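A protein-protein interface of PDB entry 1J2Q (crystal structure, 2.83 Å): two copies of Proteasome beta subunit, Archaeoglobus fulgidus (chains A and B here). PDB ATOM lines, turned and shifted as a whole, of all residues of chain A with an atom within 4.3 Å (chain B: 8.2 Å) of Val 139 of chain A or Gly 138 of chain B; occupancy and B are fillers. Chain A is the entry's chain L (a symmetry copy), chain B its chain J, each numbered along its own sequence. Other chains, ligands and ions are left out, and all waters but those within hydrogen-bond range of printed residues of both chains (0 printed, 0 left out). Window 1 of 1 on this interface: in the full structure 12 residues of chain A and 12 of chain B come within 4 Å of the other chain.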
ATOM      1  N   THR A 135      -0.535  21.072   9.689  1.00  0.00           N
ATOM      2  CA  THR A 135      -1.607  21.279  10.646  1.00  0.00           C
ATOM      3  C   THR A 135      -2.731  20.349  10.230  1.00  0.00           C
ATOM      4  O   THR A 135      -3.288  19.621  11.049  1.00  0.00           O
ATOM      5  CB  THR A 135      -2.086  22.722  10.599  1.00  0.00           C
ATOM      6  OG1 THR A 135      -1.026  23.569  11.057  1.00  0.00           O
ATOM      7  CG2 THR A 135      -3.335  22.932  11.471  1.00  0.00           C
ATOM      8  N   ALA A 136      -3.054  20.375   8.938  1.00  0.00           N
ATOM      9  CA  ALA A 136      -4.097  19.523   8.379  1.00  0.00           C
ATOM     10  C   ALA A 136      -3.810  18.066   8.735  1.00  0.00           C
ATOM     11  O   ALA A 136      -4.720  17.330   9.116  1.00  0.00           O
ATOM     12  CB  ALA A 136      -4.161  19.699   6.862  1.00  0.00           C
ATOM     13  N   TYR A 137      -2.549  17.654   8.626  1.00  0.00           N
ATOM     14  CA  TYR A 137      -2.170  16.279   8.948  1.00  0.00           C
ATOM     15  C   TYR A 137      -2.570  15.943  10.372  1.00  0.00           C
ATOM     16  O   TYR A 137      -2.874  14.791  10.693  1.00  0.00           O
ATOM     17  CB  TYR A 137      -0.660  16.073   8.789  1.00  0.00           C
ATOM     18  CG  TYR A 137      -0.255  15.521   7.446  1.00  0.00           C
ATOM     19  CD1 TYR A 137       0.470  16.291   6.538  1.00  0.00           C
ATOM     20  CD2 TYR A 137      -0.630  14.230   7.067  1.00  0.00           C
ATOM     21  CE1 TYR A 137       0.805  15.784   5.281  1.00  0.00           C
ATOM     22  CE2 TYR A 137      -0.300  13.720   5.822  1.00  0.00           C
ATOM     23  CZ  TYR A 137       0.407  14.494   4.934  1.00  0.00           C
ATOM     24  OH  TYR A 137       0.674  13.981   3.689  1.00  0.00           O
ATOM     25  N   GLY A 138      -2.553  16.966  11.224  1.00  0.00           N
ATOM     26  CA  GLY A 138      -2.921  16.796  12.613  1.00  0.00           C
ATOM     27  C   GLY A 138      -4.285  16.143  12.747  1.00  0.00           C
ATOM     28  O   GLY A 138      -4.389  15.032  13.292  1.00  0.00           O
ATOM     29  N   VAL A 139      -5.329  16.804  12.243  1.00  0.00           N
ATOM     30  CA  VAL A 139      -6.664  16.240  12.342  1.00  0.00           C
ATOM     31  C   VAL A 139      -6.845  15.001  11.456  1.00  0.00           C
ATOM     32  O   VAL A 139      -7.462  14.019  11.868  1.00  0.00           O
ATOM     33  CB  VAL A 139      -7.754  17.304  12.033  1.00  0.00           C
ATOM     34  CG1 VAL A 139      -7.106  18.662  11.814  1.00  0.00           C
ATOM     35  CG2 VAL A 139      -8.610  16.868  10.851  1.00  0.00           C
ATOM     36  N   LEU A 140      -6.298  15.025  10.250  1.00  0.00           N
ATOM     37  CA  LEU A 140      -6.448  13.865   9.382  1.00  0.00           C
ATOM     38  C   LEU A 140      -5.985  12.591  10.067  1.00  0.00           C
ATOM     39  O   LEU A 140      -6.690  11.583  10.069  1.00  0.00           O
ATOM     40  CB  LEU A 140      -5.659  14.042   8.084  1.00  0.00           C
ATOM     41  CG  LEU A 140      -6.194  15.075   7.095  1.00  0.00           C
ATOM     42  CD1 LEU A 140      -5.279  15.126   5.881  1.00  0.00           C
ATOM     43  CD2 LEU A 140      -7.634  14.704   6.684  1.00  0.00           C
ATOM     44  N   GLU A 141      -4.799  12.636  10.659  1.00  0.00           N
ATOM     45  CA  GLU A 141      -4.252  11.456  11.305  1.00  0.00           C
ATOM     46  C   GLU A 141      -4.950  11.129  12.624  1.00  0.00           C
ATOM     47  O   GLU A 141      -4.741  10.062  13.211  1.00  0.00           O
ATOM     48  CB  GLU A 141      -2.753  11.636  11.526  1.00  0.00           C
ATOM     49  CG  GLU A 141      -2.037  10.318  11.524  1.00  0.00           C
ATOM     50  CD  GLU A 141      -0.923  10.266  10.513  1.00  0.00           C
ATOM     51  OE1 GLU A 141      -0.409   9.156  10.250  1.00  0.00           O
ATOM     52  OE2 GLU A 141      -0.560  11.339   9.988  1.00  0.00           O
ATOM     53  N   ASP A 142      -5.794  12.045  13.079  1.00  0.00           N
ATOM     54  CA  ASP A 142      -6.506  11.857  14.331  1.00  0.00           C
ATOM     55  C   ASP A 142      -7.842  11.147  14.103  1.00  0.00           C
ATOM     56  O   ASP A 142      -8.122  10.117  14.714  1.00  0.00           O
ATOM     57  CB  ASP A 142      -6.748  13.224  14.993  1.00  0.00           C
ATOM     58  CG  ASP A 142      -7.462  13.117  16.331  1.00  0.00           C
ATOM     59  OD1 ASP A 142      -8.244  14.034  16.660  1.00  0.00           O
ATOM     60  OD2 ASP A 142      -7.233  12.130  17.057  1.00  0.00           O
ATOM     61  N   ARG A 143      -8.638  11.693  13.190  1.00  0.00           N
ATOM     62  CA  ARG A 143      -9.967  11.180  12.892  1.00  0.00           C
ATOM     63  C   ARG A 143     -10.126  10.163  11.758  1.00  0.00           C
ATOM     64  O   ARG A 143     -11.211   9.619  11.559  1.00  0.00           O
ATOM     65  CB  ARG A 143     -10.876  12.370  12.601  1.00  0.00           C
ATOM     66  CG  ARG A 143     -10.920  13.400  13.695  1.00  0.00           C
ATOM     67  CD  ARG A 143     -11.729  14.600  13.256  1.00  0.00           C
ATOM     68  NE  ARG A 143     -12.002  15.498  14.374  1.00  0.00           N
ATOM     69  CZ  ARG A 143     -12.739  15.171  15.435  1.00  0.00           C
ATOM     70  NH1 ARG A 143     -12.934  16.053  16.408  1.00  0.00           N
ATOM     71  NH2 ARG A 143     -13.284  13.962  15.527  1.00  0.00           N
ATOM     72  N   LEU A 156     -14.461  15.533   7.062  1.00  0.00           N
ATOM     73  CA  LEU A 156     -13.114  15.432   7.622  1.00  0.00           C
ATOM     74  C   LEU A 156     -12.156  16.371   6.903  1.00  0.00           C
ATOM     75  O   LEU A 156     -11.368  17.071   7.532  1.00  0.00           O
ATOM     76  CB  LEU A 156     -12.609  13.995   7.496  1.00  0.00           C
ATOM     77  CG  LEU A 156     -11.213  13.722   8.042  1.00  0.00           C
ATOM     78  CD1 LEU A 156     -11.059  14.395   9.402  1.00  0.00           C
ATOM     79  CD2 LEU A 156     -10.984  12.213   8.138  1.00  0.00           C
ATOM     80  N   ALA A 160     -10.089  19.440   8.488  1.00  0.00           N
ATOM     81  CA  ALA A 160      -8.644  19.593   8.474  1.00  0.00           C
ATOM     82  C   ALA A 160      -8.199  20.908   7.852  1.00  0.00           C
ATOM     83  O   ALA A 160      -7.365  21.611   8.416  1.00  0.00           O
ATOM     84  CB  ALA A 160      -8.000  18.420   7.745  1.00  0.00           C
ATOM     85  N   SER A 163      -8.704  23.771  10.233  1.00  0.00           N
ATOM     86  CA  SER A 163      -7.713  23.887  11.295  1.00  0.00           C
ATOM     87  C   SER A 163      -6.498  24.610  10.752  1.00  0.00           C
ATOM     88  O   SER A 163      -5.993  25.566  11.349  1.00  0.00           O
ATOM     89  CB  SER A 163      -7.272  22.513  11.779  1.00  0.00           C
ATOM     90  OG  SER A 163      -8.353  21.821  12.350  1.00  0.00           O
ATOM     91  N   ILE B 126      -4.892  27.665  23.902  1.00  0.00           N
ATOM     92  CA  ILE B 126      -4.127  26.615  23.241  1.00  0.00           C
ATOM     93  C   ILE B 126      -2.728  27.039  22.791  1.00  0.00           C
ATOM     94  O   ILE B 126      -2.502  28.209  22.456  1.00  0.00           O
ATOM     95  CB  ILE B 126      -4.947  26.078  22.033  1.00  0.00           C
ATOM     96  CG1 ILE B 126      -6.058  25.156  22.543  1.00  0.00           C
ATOM     97  CG2 ILE B 126      -4.064  25.299  21.076  1.00  0.00           C
ATOM     98  CD1 ILE B 126      -5.533  23.919  23.294  1.00  0.00           C
ATOM     99  N   ALA B 128       1.217  25.126  21.139  1.00  0.00           N
ATOM    100  CA  ALA B 128       2.103  24.010  20.821  1.00  0.00           C
ATOM    101  C   ALA B 128       3.469  24.609  20.535  1.00  0.00           C
ATOM    102  O   ALA B 128       3.588  25.785  20.172  1.00  0.00           O
ATOM    103  CB  ALA B 128       1.587  23.236  19.608  1.00  0.00           C
ATOM    104  N   GLY B 132       7.169  19.701  16.007  1.00  0.00           N
ATOM    105  CA  GLY B 132       5.891  19.066  15.738  1.00  0.00           C
ATOM    106  C   GLY B 132       4.685  19.952  16.028  1.00  0.00           C
ATOM    107  O   GLY B 132       3.546  19.583  15.751  1.00  0.00           O
ATOM    108  N   SER B 133       4.930  21.139  16.562  1.00  0.00           N
ATOM    109  CA  SER B 133       3.832  22.024  16.922  1.00  0.00           C
ATOM    110  C   SER B 133       2.727  22.216  15.885  1.00  0.00           C
ATOM    111  O   SER B 133       1.546  22.184  16.237  1.00  0.00           O
ATOM    112  CB  SER B 133       4.360  23.397  17.365  1.00  0.00           C
ATOM    113  OG  SER B 133       5.132  24.027  16.354  1.00  0.00           O
ATOM    114  N   LEU B 134       3.081  22.409  14.614  1.00  0.00           N
ATOM    115  CA  LEU B 134       2.063  22.639  13.575  1.00  0.00           C
ATOM    116  C   LEU B 134       1.047  21.502  13.426  1.00  0.00           C
ATOM    117  O   LEU B 134      -0.137  21.739  13.149  1.00  0.00           O
ATOM    118  CB  LEU B 134       2.738  22.922  12.231  1.00  0.00           C
ATOM    119  CG  LEU B 134       3.606  24.196  12.187  1.00  0.00           C
ATOM    120  CD1 LEU B 134       4.187  24.367  10.791  1.00  0.00           C
ATOM    121  CD2 LEU B 134       2.787  25.424  12.567  1.00  0.00           C
ATOM    122  N   THR B 135       1.513  20.267  13.599  1.00  0.00           N
ATOM    123  CA  THR B 135       0.629  19.117  13.508  1.00  0.00           C
ATOM    124  C   THR B 135      -0.218  19.086  14.781  1.00  0.00           C
ATOM    125  O   THR B 135      -1.447  18.960  14.728  1.00  0.00           O
ATOM    126  CB  THR B 135       1.421  17.815  13.390  1.00  0.00           C
ATOM    127  OG1 THR B 135       2.170  17.828  12.173  1.00  0.00           O
ATOM    128  CG2 THR B 135       0.486  16.623  13.389  1.00  0.00           C
ATOM    129  N   ALA B 136       0.447  19.221  15.928  1.00  0.00           N
ATOM    130  CA  ALA B 136      -0.234  19.225  17.205  1.00  0.00           C
ATOM    131  C   ALA B 136      -1.334  20.275  17.160  1.00  0.00           C
ATOM    132  O   ALA B 136      -2.477  20.004  17.531  1.00  0.00           O
ATOM    133  CB  ALA B 136       0.739  19.529  18.293  1.00  0.00           C
ATOM    134  N   TYR B 137      -0.996  21.473  16.693  1.00  0.00           N
ATOM    135  CA  TYR B 137      -1.975  22.553  16.589  1.00  0.00           C
ATOM    136  C   TYR B 137      -3.226  22.090  15.850  1.00  0.00           C
ATOM    137  O   TYR B 137      -4.335  22.558  16.118  1.00  0.00           O
ATOM    138  CB  TYR B 137      -1.370  23.744  15.855  1.00  0.00           C
ATOM    139  CG  TYR B 137      -0.756  24.767  16.769  1.00  0.00           C
ATOM    140  CD1 TYR B 137       0.613  24.999  16.773  1.00  0.00           C
ATOM    141  CD2 TYR B 137      -1.560  25.520  17.642  1.00  0.00           C
ATOM    142  CE1 TYR B 137       1.171  25.963  17.626  1.00  0.00           C
ATOM    143  CE2 TYR B 137      -1.015  26.477  18.490  1.00  0.00           C
ATOM    144  CZ  TYR B 137       0.346  26.692  18.477  1.00  0.00           C
ATOM    145  OH  TYR B 137       0.885  27.629  19.315  1.00  0.00           O
ATOM    146  N   GLY B 138      -3.041  21.167  14.917  1.00  0.00           N
ATOM    147  CA  GLY B 138      -4.165  20.662  14.162  1.00  0.00           C
ATOM    148  C   GLY B 138      -5.260  20.120  15.056  1.00  0.00           C
ATOM    149  O   GLY B 138      -6.382  20.638  15.043  1.00  0.00           O
ATOM    150  N   VAL B 139      -4.942  19.086  15.834  1.00  0.00           N
ATOM    151  CA  VAL B 139      -5.942  18.501  16.715  1.00  0.00           C
ATOM    152  C   VAL B 139      -6.334  19.460  17.838  1.00  0.00           C
ATOM    153  O   VAL B 139      -7.511  19.550  18.193  1.00  0.00           O
ATOM    154  CB  VAL B 139      -5.486  17.127  17.308  1.00  0.00           C
ATOM    155  CG1 VAL B 139      -4.127  16.722  16.757  1.00  0.00           C
ATOM    156  CG2 VAL B 139      -5.483  17.176  18.799  1.00  0.00           C
ATOM    157  N   LEU B 140      -5.370  20.195  18.387  1.00  0.00           N
ATOM    158  CA  LEU B 140      -5.695  21.135  19.451  1.00  0.00           C
ATOM    159  C   LEU B 140      -6.763  22.115  19.002  1.00  0.00           C
ATOM    160  O   LEU B 140      -7.744  22.332  19.703  1.00  0.00           O
ATOM    161  CB  LEU B 140      -4.464  21.921  19.896  1.00  0.00           C
ATOM    162  CG  LEU B 140      -3.427  21.161  20.718  1.00  0.00           C
ATOM    163  CD1 LEU B 140      -2.276  22.086  21.073  1.00  0.00           C
ATOM    164  CD2 LEU B 140      -4.078  20.622  21.978  1.00  0.00           C
ATOM    165  N   GLU B 141      -6.590  22.699  17.824  1.00  0.00           N
ATOM    166  CA  GLU B 141      -7.570  23.671  17.368  1.00  0.00           C
ATOM    167  C   GLU B 141      -8.882  23.029  16.904  1.00  0.00           C
ATOM    168  O   GLU B 141      -9.889  23.706  16.677  1.00  0.00           O
ATOM    169  CB  GLU B 141      -6.976  24.545  16.259  1.00  0.00           C
ATOM    170  CG  GLU B 141      -7.557  25.958  16.276  1.00  0.00           C
ATOM    171  CD  GLU B 141      -6.499  27.040  16.426  1.00  0.00           C
ATOM    172  OE1 GLU B 141      -6.856  28.215  16.673  1.00  0.00           O
ATOM    173  OE2 GLU B 141      -5.304  26.713  16.286  1.00  0.00           O
ATOM    174  N   ASP B 142      -8.874  21.709  16.796  1.00  0.00           N
ATOM    175  CA  ASP B 142     -10.043  20.977  16.350  1.00  0.00           C
ATOM    176  C   ASP B 142     -10.944  20.593  17.523  1.00  0.00           C
ATOM    177  O   ASP B 142     -12.149  20.862  17.520  1.00  0.00           O
ATOM    178  CB  ASP B 142      -9.583  19.717  15.620  1.00  0.00           C
ATOM    179  CG  ASP B 142     -10.725  18.932  15.015  1.00  0.00           C
ATOM    180  OD1 ASP B 142     -10.567  17.692  14.886  1.00  0.00           O
ATOM    181  OD2 ASP B 142     -11.758  19.551  14.659  1.00  0.00           O
ATOM    182  N   ARG B 143     -10.341  19.977  18.534  1.00  0.00           N
ATOM    183  CA  ARG B 143     -11.066  19.503  19.706  1.00  0.00           C
ATOM    184  C   ARG B 143     -11.162  20.399  20.950  1.00  0.00           C
ATOM    185  O   ARG B 143     -11.891  20.072  21.885  1.00  0.00           O
ATOM    186  CB  ARG B 143     -10.475  18.169  20.123  1.00  0.00           C
ATOM    187  CG  ARG B 143     -10.479  17.151  19.034  1.00  0.00           C
ATOM    188  CD  ARG B 143      -9.736  15.925  19.487  1.00  0.00           C
ATOM    189  NE  ARG B 143      -9.926  14.800  18.578  1.00  0.00           N
ATOM    190  CZ  ARG B 143     -11.104  14.240  18.329  1.00  0.00           C
ATOM    191  NH1 ARG B 143     -11.197  13.212  17.487  1.00  0.00           N
ATOM    192  NH2 ARG B 143     -12.187  14.719  18.929  1.00  0.00           N
ATOM    193  N   PHE B 144     -10.445  21.512  20.983  1.00  0.00           N
ATOM    194  CA  PHE B 144     -10.489  22.372  22.162  1.00  0.00           C
ATOM    195  C   PHE B 144     -11.715  23.269  22.283  1.00  0.00           C
ATOM    196  O   PHE B 144     -12.249  23.761  21.292  1.00  0.00           O
ATOM    197  CB  PHE B 144      -9.242  23.253  22.221  1.00  0.00           C
ATOM    198  CG  PHE B 144      -9.243  24.237  23.362  1.00  0.00           C
ATOM    199  CD1 PHE B 144      -8.694  23.892  24.605  1.00  0.00           C
ATOM    200  CD2 PHE B 144      -9.780  25.511  23.199  1.00  0.00           C
ATOM    201  CE1 PHE B 144      -8.682  24.810  25.663  1.00  0.00           C
ATOM    202  CE2 PHE B 144      -9.771  26.426  24.255  1.00  0.00           C
ATOM    203  CZ  PHE B 144      -9.218  26.072  25.486  1.00  0.00           C
ATOM    204  N   LEU B 156      -6.575  15.205  25.473  1.00  0.00           N
ATOM    205  CA  LEU B 156      -6.400  16.019  24.290  1.00  0.00           C
ATOM    206  C   LEU B 156      -4.913  16.214  24.010  1.00  0.00           C
ATOM    207  O   LEU B 156      -4.446  16.019  22.884  1.00  0.00           O
ATOM    208  CB  LEU B 156      -7.082  17.378  24.493  1.00  0.00           C
ATOM    209  CG  LEU B 156      -6.981  18.367  23.331  1.00  0.00           C
ATOM    210  CD1 LEU B 156      -7.261  17.647  22.032  1.00  0.00           C
ATOM    211  CD2 LEU B 156      -7.961  19.531  23.536  1.00  0.00           C
ATOM    212  N   ALA B 160      -2.900  15.206  20.690  1.00  0.00           N
ATOM    213  CA  ALA B 160      -2.144  16.084  19.794  1.00  0.00           C
ATOM    214  C   ALA B 160      -0.693  15.634  19.583  1.00  0.00           C
ATOM    215  O   ALA B 160      -0.243  15.468  18.448  1.00  0.00           O
ATOM    216  CB  ALA B 160      -2.179  17.514  20.320  1.00  0.00           C
ATOM    217  N   SER B 163      -0.381  12.678  17.350  1.00  0.00           N
ATOM    218  CA  SER B 163      -0.525  12.967  15.928  1.00  0.00           C
ATOM    219  C   SER B 163       0.818  13.467  15.417  1.00  0.00           C
ATOM    220  O   SER B 163       1.345  12.991  14.409  1.00  0.00           O
ATOM    221  CB  SER B 163      -1.577  14.057  15.698  1.00  0.00           C
ATOM    222  OG  SER B 163      -2.876  13.626  16.066  1.00  0.00           O
ATOM    223  N   ALA B 164       1.369  14.429  16.139  1.00  0.00           N
ATOM    224  CA  ALA B 164       2.641  15.027  15.779  1.00  0.00           C
ATOM    225  C   ALA B 164       3.756  14.022  15.607  1.00  0.00           C
ATOM    226  O   ALA B 164       4.544  14.136  14.685  1.00  0.00           O
ATOM    227  CB  ALA B 164       3.044  16.074  16.819  1.00  0.00           C
ATOM    228  N   LYS B 166       3.575  11.312  14.503  1.00  0.00           N
ATOM    229  CA  LYS B 166       3.321  10.607  13.260  1.00  0.00           C
ATOM    230  C   LYS B 166       3.846  11.301  11.997  1.00  0.00           C
ATOM    231  O   LYS B 166       3.994  10.655  10.959  1.00  0.00           O
ATOM    232  CB  LYS B 166       1.817  10.377  13.108  1.00  0.00           C
ATOM    233  CG  LYS B 166       1.224   9.326  14.028  1.00  0.00           C
ATOM    234  CD  LYS B 166      -0.295   9.431  13.974  1.00  0.00           C
ATOM    235  CE  LYS B 166      -1.020   8.295  14.694  1.00  0.00           C
ATOM    236  NZ  LYS B 166      -2.496   8.562  14.701  1.00  0.00           N
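Ala 136 of chain A touches none of the printed residues of chain B. Gly 138 of chain A touches just these residues of chain B: Thr 135 (3.4 Å), Val 139 (3.9 Å) and Ser 163 (3.5 Å). Of chain B, only Gly 138 comes within 4 Å of Val 139 of chain A. Of the printed residues of chain B, Arg 143 of chain A touches Asp 142 and Arg 143. Printed residues of chain B within 4 Å of Ser 163 of chain A: Gly 138. Printed residues of chain A within 4 Å of Val 139 of chain B: Gly 138 (3.9 Å). Of the printed residues of chain A, Arg 143 of chain B touches Asp 142 (2.7 Å) and Arg 143 (2.9 Å). Printed residues of chain A within 4 Å of Ser 163 of chain B: Gly 138.
Printed residues of chain B that touch a printed residue of chain A: Leu 134, Thr 135, Gly 138, Val 139, Asp 142, Arg 143, Ser 163 and Lys 166. Hydrophobic or aromatic side chains of chain B within 4 Å of the printed part of chain A: Leu 134 and Val 139. Hydrophobic or aromatic side chains of chain A that line the printed part of chain B: Val 139. Among the printed residues, 11 pairs touch across the chains.
Thr 135 of chain A touches Gly 138 of chain B, and with the chains exchanged Gly 138 of chain A touches Thr 135 of chain B. Gly 138 of chain A touches Val 139 of chain B, and with the chains exchanged Val 139 of chain A touches Gly 138 of chain B. Gly 138 of chain A touches Ser 163 of chain B, and with the chains exchanged Ser 163 of chain A touches Gly 138 of chain B. Arg 143 of chain A touches its own counterpart, Arg 143 of chain B. Of the 11 pairs that touch across the chains among the printed residues, 9 have their exchanged pair printed and touching as well.
O of Leu 134 of chain B lies within hydrogen-bond range of OG1 of Thr 135 of chain A. NE of Arg 143 of chain A is in salt-bridge range of OD1 of Asp 142 of chain B, 2.7 Å away. OD1 of Asp 142 of chain A lies within salt-bridge range of NE of Arg 143 of chain B, at 2.7 Å. O of Gly 138 of chain A is in hydrogen-bond range of OG of Ser 163 of chain B (3.5 Å). The side-chain amino group (NZ) of Lys 166 of chain B lies within hydrogen-bond range of the backbone carbonyl oxygen (O) of Glu 141 of chain A. NH1 of Arg 143 of chain A lies close to NH2 of Arg 143 of chain B (2.9 Å).
Among the printed residues, pairs that only touch across the chains: Thr 135 of chain A with Gly 138 of chain B, Gly 138 of chain A with Thr 135 of chain B, Gly 138 of chain A with Val 139 of chain B, Val 139 of chain A with Gly 138 of chain B and Ser 163 of chain A with Gly 138 of chain B.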
